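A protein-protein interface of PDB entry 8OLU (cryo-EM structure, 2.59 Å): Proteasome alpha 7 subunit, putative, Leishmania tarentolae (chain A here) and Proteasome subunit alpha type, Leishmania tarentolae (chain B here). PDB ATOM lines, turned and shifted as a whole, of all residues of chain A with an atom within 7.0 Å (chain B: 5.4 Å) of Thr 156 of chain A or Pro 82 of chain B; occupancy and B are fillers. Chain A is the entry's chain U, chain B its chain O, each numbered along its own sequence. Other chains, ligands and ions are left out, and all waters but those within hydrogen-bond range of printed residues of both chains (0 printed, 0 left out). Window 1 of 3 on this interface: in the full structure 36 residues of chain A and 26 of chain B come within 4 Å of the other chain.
A ring nitrogen (NE2) of His 121 of chain A lies close to the backbone carbonyl oxygen (O) of Pro 82 of chain B, 3.5 Å away.
NH2 of Arg 85 of chain B lies within salt-bridge range of OE2 of Glu 118 of chain A, 3.3 Å away.
NE2 of His 121 of chain A lies close to OD1 of Asp 83 of chain B.
The guanidinium group (NE) of Arg 80 of chain B lies within salt-bridge range of the side-chain carboxylate (OD1) of Asp 83 of chain B.
O of His 121 of chain A sits at hydrogen-bond distance from OG1 of Thr 124 of chain A (2.6 Å).
The backbone NH (N) of Ser 154 of chain A is in hydrogen-bond range of the side-chain carboxylate (OD2) of Asp 152 of chain A, at 2.7 Å.
The side-chain carboxylate (OD2) of Asp 152 of chain A sits at hydrogen-bond distance from the backbone NH (N) of Gly 155 of chain A (3.3 Å).
N of Thr 156 of chain A sits at hydrogen-bond distance from OD2 of Asp 152 of chain A (3.5 Å).
The side-chain hydroxyl (OG1) of Thr 156 of chain A sits at hydrogen-bond distance from the side-chain hydroxyl (OG) of Ser 154 of chain A, at 3.0 Å.
Among the printed residues, pairs that only touch across the chains: Thr 156 of chain A with Pro 82 of chain B (3.3 Å), Ser 154 of chain A with Pro 82 of chain B (3.5 Å), His 121 of chain A with Ala 86 of chain B (3.6 Å) and Gly 155 of chain A with Pro 82 of chain B (3.7 Å).
Printed residues of chain A that touch a printed residue of chain B: Glu 118, His 121, Ser 154, Gly 155 and Thr 156.
Hydrophobic or aromatic side chains of chain A within 4 Å of the printed part of chain B: His 121.
Along chain A the printed residues that touch a printed residue of chain B span positions 118 to 156.
Of the 8 printed residues of chain B, 4 touch a printed residue of chain A.
Printed residues of chain B that touch a printed residue of chain A: Pro 82, Asp 83, Arg 85 and Ala 86.
Among the printed residues, 7 pairs touch across the chains.
Thr 156 of chain A touches just one residue of chain B: Pro 82 (3.3 Å).
Pro 82 of chain B touches just these residues of chain A: His 121 (3.4 Å), Ser 154 (3.5 Å), Gly 155 (3.7 Å) and Thr 156 (3.3 Å).
Of the printed residues of chain B, Ser 154 of chain A touches Pro 82.
Of the printed residues of chain A, Asp 83 of chain B touches His 121 (2.4 Å).
Printed residues of chain B within 4 Å of Glu 118 of chain A: Arg 85.
Ser 151 of chain A touches none of the printed residues of chain B.
The nearest residue of chain B that does not touch Thr 156 of chain A is Ala 81 of chain B (4.6 Å).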
ATOM      1  N   ALA A 113     -24.429 -30.709  -5.230  1.00  0.00           N
ATOM      2  CA  ALA A 113     -23.755 -29.732  -4.423  1.00  0.00           C
ATOM      3  C   ALA A 113     -22.395 -29.396  -4.965  1.00  0.00           C
ATOM      4  O   ALA A 113     -21.860 -28.339  -4.763  1.00  0.00           O
ATOM      5  CB  ALA A 113     -23.611 -30.311  -3.073  1.00  0.00           C
ATOM      6  N   GLY A 117     -21.309 -25.682  -6.025  1.00  0.00           N
ATOM      7  CA  GLY A 117     -20.055 -25.126  -5.566  1.00  0.00           C
ATOM      8  C   GLY A 117     -19.150 -24.614  -6.658  1.00  0.00           C
ATOM      9  O   GLY A 117     -18.539 -23.600  -6.498  1.00  0.00           O
ATOM     10  N   GLU A 118     -19.068 -25.348  -7.739  1.00  0.00           N
ATOM     11  CA  GLU A 118     -18.247 -25.005  -8.874  1.00  0.00           C
ATOM     12  C   GLU A 118     -18.742 -23.702  -9.445  1.00  0.00           C
ATOM     13  O   GLU A 118     -17.969 -22.832  -9.803  1.00  0.00           O
ATOM     14  CB  GLU A 118     -18.320 -26.075  -9.955  1.00  0.00           C
ATOM     15  CG  GLU A 118     -17.601 -27.403  -9.596  1.00  0.00           C
ATOM     16  CD  GLU A 118     -17.984 -28.688 -10.397  1.00  0.00           C
ATOM     17  OE1 GLU A 118     -18.530 -28.565 -11.596  1.00  0.00           O
ATOM     18  OE2 GLU A 118     -17.769 -29.859  -9.834  1.00  0.00           O
ATOM     19  N   MET A 120     -20.705 -21.384  -7.882  1.00  0.00           N
ATOM     20  CA  MET A 120     -20.355 -20.310  -6.996  1.00  0.00           C
ATOM     21  C   MET A 120     -18.895 -19.995  -7.049  1.00  0.00           C
ATOM     22  O   MET A 120     -18.531 -18.857  -6.949  1.00  0.00           O
ATOM     23  CB  MET A 120     -20.745 -20.633  -5.560  1.00  0.00           C
ATOM     24  CG  MET A 120     -22.253 -20.636  -5.481  1.00  0.00           C
ATOM     25  SD  MET A 120     -22.904 -21.322  -3.981  1.00  0.00           S
ATOM     26  CE  MET A 120     -22.852 -19.804  -3.061  1.00  0.00           C
ATOM     27  N   HIS A 121     -18.023 -20.964  -7.121  1.00  0.00           N
ATOM     28  CA  HIS A 121     -16.611 -20.617  -7.070  1.00  0.00           C
ATOM     29  C   HIS A 121     -16.211 -19.834  -8.296  1.00  0.00           C
ATOM     30  O   HIS A 121     -15.411 -18.936  -8.235  1.00  0.00           O
ATOM     31  CB  HIS A 121     -15.771 -21.864  -6.914  1.00  0.00           C
ATOM     32  CG  HIS A 121     -14.349 -21.713  -7.264  1.00  0.00           C
ATOM     33  ND1 HIS A 121     -13.876 -21.908  -8.534  1.00  0.00           N
ATOM     34  CD2 HIS A 121     -13.306 -21.440  -6.457  1.00  0.00           C
ATOM     35  CE1 HIS A 121     -12.558 -21.717  -8.521  1.00  0.00           C
ATOM     36  NE2 HIS A 121     -12.192 -21.380  -7.237  1.00  0.00           N
ATOM     37  N   THR A 124     -15.654 -16.320  -8.121  1.00  0.00           N
ATOM     38  CA  THR A 124     -14.616 -15.787  -7.271  1.00  0.00           C
ATOM     39  C   THR A 124     -13.291 -15.752  -7.958  1.00  0.00           C
ATOM     40  O   THR A 124     -12.300 -15.606  -7.292  1.00  0.00           O
ATOM     41  CB  THR A 124     -14.411 -16.662  -6.046  1.00  0.00           C
ATOM     42  OG1 THR A 124     -13.939 -17.980  -6.314  1.00  0.00           O
ATOM     43  CG2 THR A 124     -15.722 -16.775  -5.323  1.00  0.00           C
ATOM     44  N   VAL A 150     -23.721 -27.757   2.269  1.00  0.00           N
ATOM     45  CA  VAL A 150     -23.758 -26.309   2.155  1.00  0.00           C
ATOM     46  C   VAL A 150     -22.653 -25.832   1.266  1.00  0.00           C
ATOM     47  O   VAL A 150     -21.504 -26.123   1.578  1.00  0.00           O
ATOM     48  CB  VAL A 150     -23.529 -25.617   3.479  1.00  0.00           C
ATOM     49  CG1 VAL A 150     -23.470 -24.157   3.179  1.00  0.00           C
ATOM     50  CG2 VAL A 150     -24.620 -25.901   4.459  1.00  0.00           C
ATOM     51  N   SER A 151     -22.995 -25.011   0.283  1.00  0.00           N
ATOM     52  CA  SER A 151     -22.058 -24.265  -0.544  1.00  0.00           C
ATOM     53  C   SER A 151     -22.043 -22.817  -0.124  1.00  0.00           C
ATOM     54  O   SER A 151     -23.070 -22.158  -0.218  1.00  0.00           O
ATOM     55  CB  SER A 151     -22.532 -24.349  -1.954  1.00  0.00           C
ATOM     56  OG  SER A 151     -21.588 -23.806  -2.878  1.00  0.00           O
ATOM     57  N   ASP A 152     -20.888 -22.291   0.284  1.00  0.00           N
ATOM     58  CA  ASP A 152     -20.789 -20.913   0.743  1.00  0.00           C
ATOM     59  C   ASP A 152     -20.345 -20.052  -0.427  1.00  0.00           C
ATOM     60  O   ASP A 152     -20.128 -20.548  -1.517  1.00  0.00           O
ATOM     61  CB  ASP A 152     -19.946 -20.846   2.009  1.00  0.00           C
ATOM     62  CG  ASP A 152     -18.461 -20.911   1.750  1.00  0.00           C
ATOM     63  OD1 ASP A 152     -17.694 -21.109   2.729  1.00  0.00           O
ATOM     64  OD2 ASP A 152     -18.064 -20.704   0.589  1.00  0.00           O
ATOM     65  N   PRO A 153     -20.229 -18.722  -0.284  1.00  0.00           N
ATOM     66  CA  PRO A 153     -19.816 -17.879  -1.386  1.00  0.00           C
ATOM     67  C   PRO A 153     -18.448 -18.119  -1.990  1.00  0.00           C
ATOM     68  O   PRO A 153     -18.203 -17.683  -3.105  1.00  0.00           O
ATOM     69  CB  PRO A 153     -19.677 -16.509  -0.773  1.00  0.00           C
ATOM     70  CG  PRO A 153     -20.580 -16.549   0.358  1.00  0.00           C
ATOM     71  CD  PRO A 153     -20.405 -17.936   0.945  1.00  0.00           C
ATOM     72  N   SER A 154     -17.551 -18.728  -1.251  1.00  0.00           N
ATOM     73  CA  SER A 154     -16.298 -19.109  -1.826  1.00  0.00           C
ATOM     74  C   SER A 154     -16.452 -20.281  -2.775  1.00  0.00           C
ATOM     75  O   SER A 154     -15.539 -20.607  -3.511  1.00  0.00           O
ATOM     76  CB  SER A 154     -15.415 -19.502  -0.736  1.00  0.00           C
ATOM     77  OG  SER A 154     -15.863 -20.742  -0.201  1.00  0.00           O
ATOM     78  N   GLY A 155     -17.558 -21.007  -2.661  1.00  0.00           N
ATOM     79  CA  GLY A 155     -17.804 -22.204  -3.445  1.00  0.00           C
ATOM     80  C   GLY A 155     -17.384 -23.462  -2.702  1.00  0.00           C
ATOM     81  O   GLY A 155     -17.349 -24.538  -3.282  1.00  0.00           O
ATOM     82  N   THR A 156     -16.965 -23.300  -1.454  1.00  0.00           N
ATOM     83  CA  THR A 156     -16.564 -24.434  -0.659  1.00  0.00           C
ATOM     84  C   THR A 156     -17.806 -25.200  -0.274  1.00  0.00           C
ATOM     85  O   THR A 156     -18.801 -24.600   0.087  1.00  0.00           O
ATOM     86  CB  THR A 156     -15.931 -24.004   0.654  1.00  0.00           C
ATOM     87  OG1 THR A 156     -14.652 -23.423   0.416  1.00  0.00           O
ATOM     88  CG2 THR A 156     -15.710 -25.201   1.563  1.00  0.00           C
ATOM     89  N   VAL A 157     -17.772 -26.510  -0.341  1.00  0.00           N
ATOM     90  CA  VAL A 157     -18.984 -27.296  -0.184  1.00  0.00           C
ATOM     91  C   VAL A 157     -18.717 -28.288   0.907  1.00  0.00           C
ATOM     92  O   VAL A 157     -17.654 -28.882   0.918  1.00  0.00           O
ATOM     93  CB  VAL A 157     -19.242 -28.073  -1.458  1.00  0.00           C
ATOM     94  CG1 VAL A 157     -20.235 -29.183  -1.226  1.00  0.00           C
ATOM     95  CG2 VAL A 157     -19.668 -27.169  -2.593  1.00  0.00           C
ATOM     96  N   ALA A 158     -19.653 -28.504   1.794  1.00  0.00           N
ATOM     97  CA  ALA A 158     -19.368 -29.486   2.834  1.00  0.00           C
ATOM     98  C   ALA A 158     -20.625 -30.248   3.175  1.00  0.00           C
ATOM     99  O   ALA A 158     -21.696 -29.682   3.085  1.00  0.00           O
ATOM    100  CB  ALA A 158     -18.822 -28.753   4.017  1.00  0.00           C
ATOM    101  N   TYR A 160     -23.154 -32.074   5.847  1.00  0.00           N
ATOM    102  CA  TYR A 160     -23.358 -31.939   7.252  1.00  0.00           C
ATOM    103  C   TYR A 160     -24.436 -32.902   7.695  1.00  0.00           C
ATOM    104  O   TYR A 160     -25.287 -33.280   6.916  1.00  0.00           O
ATOM    105  CB  TYR A 160     -23.803 -30.522   7.577  1.00  0.00           C
ATOM    106  CG  TYR A 160     -22.776 -29.458   7.346  1.00  0.00           C
ATOM    107  CD1 TYR A 160     -22.104 -28.901   8.412  1.00  0.00           C
ATOM    108  CD2 TYR A 160     -22.551 -28.923   6.090  1.00  0.00           C
ATOM    109  CE1 TYR A 160     -21.146 -27.913   8.234  1.00  0.00           C
ATOM    110  CE2 TYR A 160     -21.621 -27.906   5.881  1.00  0.00           C
ATOM    111  CZ  TYR A 160     -20.910 -27.409   6.966  1.00  0.00           C
ATOM    112  OH  TYR A 160     -19.973 -26.419   6.845  1.00  0.00           O
ATOM    113  N   ARG B  80      -6.655 -23.619  -1.197  1.00  0.00           N
ATOM    114  CA  ARG B  80      -7.992 -23.092  -1.239  1.00  0.00           C
ATOM    115  C   ARG B  80      -8.886 -24.163  -1.861  1.00  0.00           C
ATOM    116  O   ARG B  80      -8.743 -24.505  -3.038  1.00  0.00           O
ATOM    117  CB  ARG B  80      -7.916 -21.768  -1.998  1.00  0.00           C
ATOM    118  CG  ARG B  80      -9.125 -20.898  -1.747  1.00  0.00           C
ATOM    119  CD  ARG B  80      -9.208 -19.824  -2.809  1.00  0.00           C
ATOM    120  NE  ARG B  80     -10.416 -19.046  -2.613  1.00  0.00           N
ATOM    121  CZ  ARG B  80     -10.632 -18.270  -1.557  1.00  0.00           C
ATOM    122  NH1 ARG B  80      -9.687 -18.079  -0.643  1.00  0.00           N
ATOM    123  NH2 ARG B  80     -11.835 -17.732  -1.443  1.00  0.00           N
ATOM    124  N   ALA B  81      -9.774 -24.726  -1.024  1.00  0.00           N
ATOM    125  CA  ALA B  81     -10.363 -25.996  -1.389  1.00  0.00           C
ATOM    126  C   ALA B  81     -11.150 -25.901  -2.702  1.00  0.00           C
ATOM    127  O   ALA B  81     -11.068 -26.750  -3.601  1.00  0.00           O
ATOM    128  CB  ALA B  81     -11.231 -26.488  -0.294  1.00  0.00           C
ATOM    129  N   PRO B  82     -11.998 -24.891  -2.835  1.00  0.00           N
ATOM    130  CA  PRO B  82     -12.800 -24.777  -4.035  1.00  0.00           C
ATOM    131  C   PRO B  82     -11.959 -24.493  -5.259  1.00  0.00           C
ATOM    132  O   PRO B  82     -12.384 -24.761  -6.381  1.00  0.00           O
ATOM    133  CB  PRO B  82     -13.753 -23.631  -3.670  1.00  0.00           C
ATOM    134  CG  PRO B  82     -13.009 -22.852  -2.634  1.00  0.00           C
ATOM    135  CD  PRO B  82     -12.327 -23.913  -1.803  1.00  0.00           C
ATOM    136  N   ASP B  83     -10.788 -23.904  -5.080  1.00  0.00           N
ATOM    137  CA  ASP B  83      -9.910 -23.723  -6.217  1.00  0.00           C
ATOM    138  C   ASP B  83      -9.370 -25.081  -6.566  1.00  0.00           C
ATOM    139  O   ASP B  83      -9.208 -25.403  -7.719  1.00  0.00           O
ATOM    140  CB  ASP B  83      -8.756 -22.764  -5.904  1.00  0.00           C
ATOM    141  CG  ASP B  83      -9.076 -21.277  -5.764  1.00  0.00           C
ATOM    142  OD1 ASP B  83     -10.266 -20.891  -5.942  1.00  0.00           O
ATOM    143  OD2 ASP B  83      -8.119 -20.487  -5.517  1.00  0.00           O
ATOM    144  N   GLY B  84      -9.111 -25.908  -5.571  1.00  0.00           N
ATOM    145  CA  GLY B  84      -8.661 -27.263  -5.874  1.00  0.00           C
ATOM    146  C   GLY B  84      -9.727 -28.035  -6.617  1.00  0.00           C
ATOM    147  O   GLY B  84      -9.482 -28.700  -7.578  1.00  0.00           O
ATOM    148  N   ARG B  85     -10.948 -27.881  -6.180  1.00  0.00           N
ATOM    149  CA  ARG B  85     -12.027 -28.601  -6.797  1.00  0.00           C
ATOM    150  C   ARG B  85     -12.132 -28.187  -8.235  1.00  0.00           C
ATOM    151  O   ARG B  85     -12.469 -28.984  -9.097  1.00  0.00           O
ATOM    152  CB  ARG B  85     -13.303 -28.349  -6.018  1.00  0.00           C
ATOM    153  CG  ARG B  85     -14.503 -29.075  -6.574  1.00  0.00           C
ATOM    154  CD  ARG B  85     -14.433 -30.545  -6.185  1.00  0.00           C
ATOM    155  NE  ARG B  85     -15.000 -31.328  -7.306  1.00  0.00           N
ATOM    156  CZ  ARG B  85     -15.982 -32.217  -7.210  1.00  0.00           C
ATOM    157  NH1 ARG B  85     -16.206 -32.847  -6.068  1.00  0.00           N
ATOM    158  NH2 ARG B  85     -16.665 -32.520  -8.298  1.00  0.00           N
ATOM    159  N   ALA B  86     -11.868 -26.935  -8.502  1.00  0.00           N
ATOM    160  CA  ALA B  86     -11.974 -26.478  -9.857  1.00  0.00           C
ATOM    161  C   ALA B  86     -10.832 -27.030 -10.665  1.00  0.00           C
ATOM    162  O   ALA B  86     -11.031 -27.354 -11.841  1.00  0.00           O
ATOM    163  CB  ALA B  86     -11.954 -25.001  -9.904  1.00  0.00           C
ATOM    164  N   LEU B  87      -9.629 -27.052 -10.111  1.00  0.00           N
ATOM    165  CA  LEU B  87      -8.587 -27.642 -10.923  1.00  0.00           C
ATOM    166  C   LEU B  87      -8.880 -29.101 -11.219  1.00  0.00           C
ATOM    167  O   LEU B  87      -8.456 -29.645 -12.235  1.00  0.00           O
ATOM    168  CB  LEU B  87      -7.263 -27.574 -10.194  1.00  0.00           C
ATOM    169  CG  LEU B  87      -6.631 -26.202 -10.239  1.00  0.00           C
ATOM    170  CD1 LEU B  87      -5.273 -26.238  -9.648  1.00  0.00           C
ATOM    171  CD2 LEU B  87      -6.556 -25.741 -11.663  1.00  0.00           C
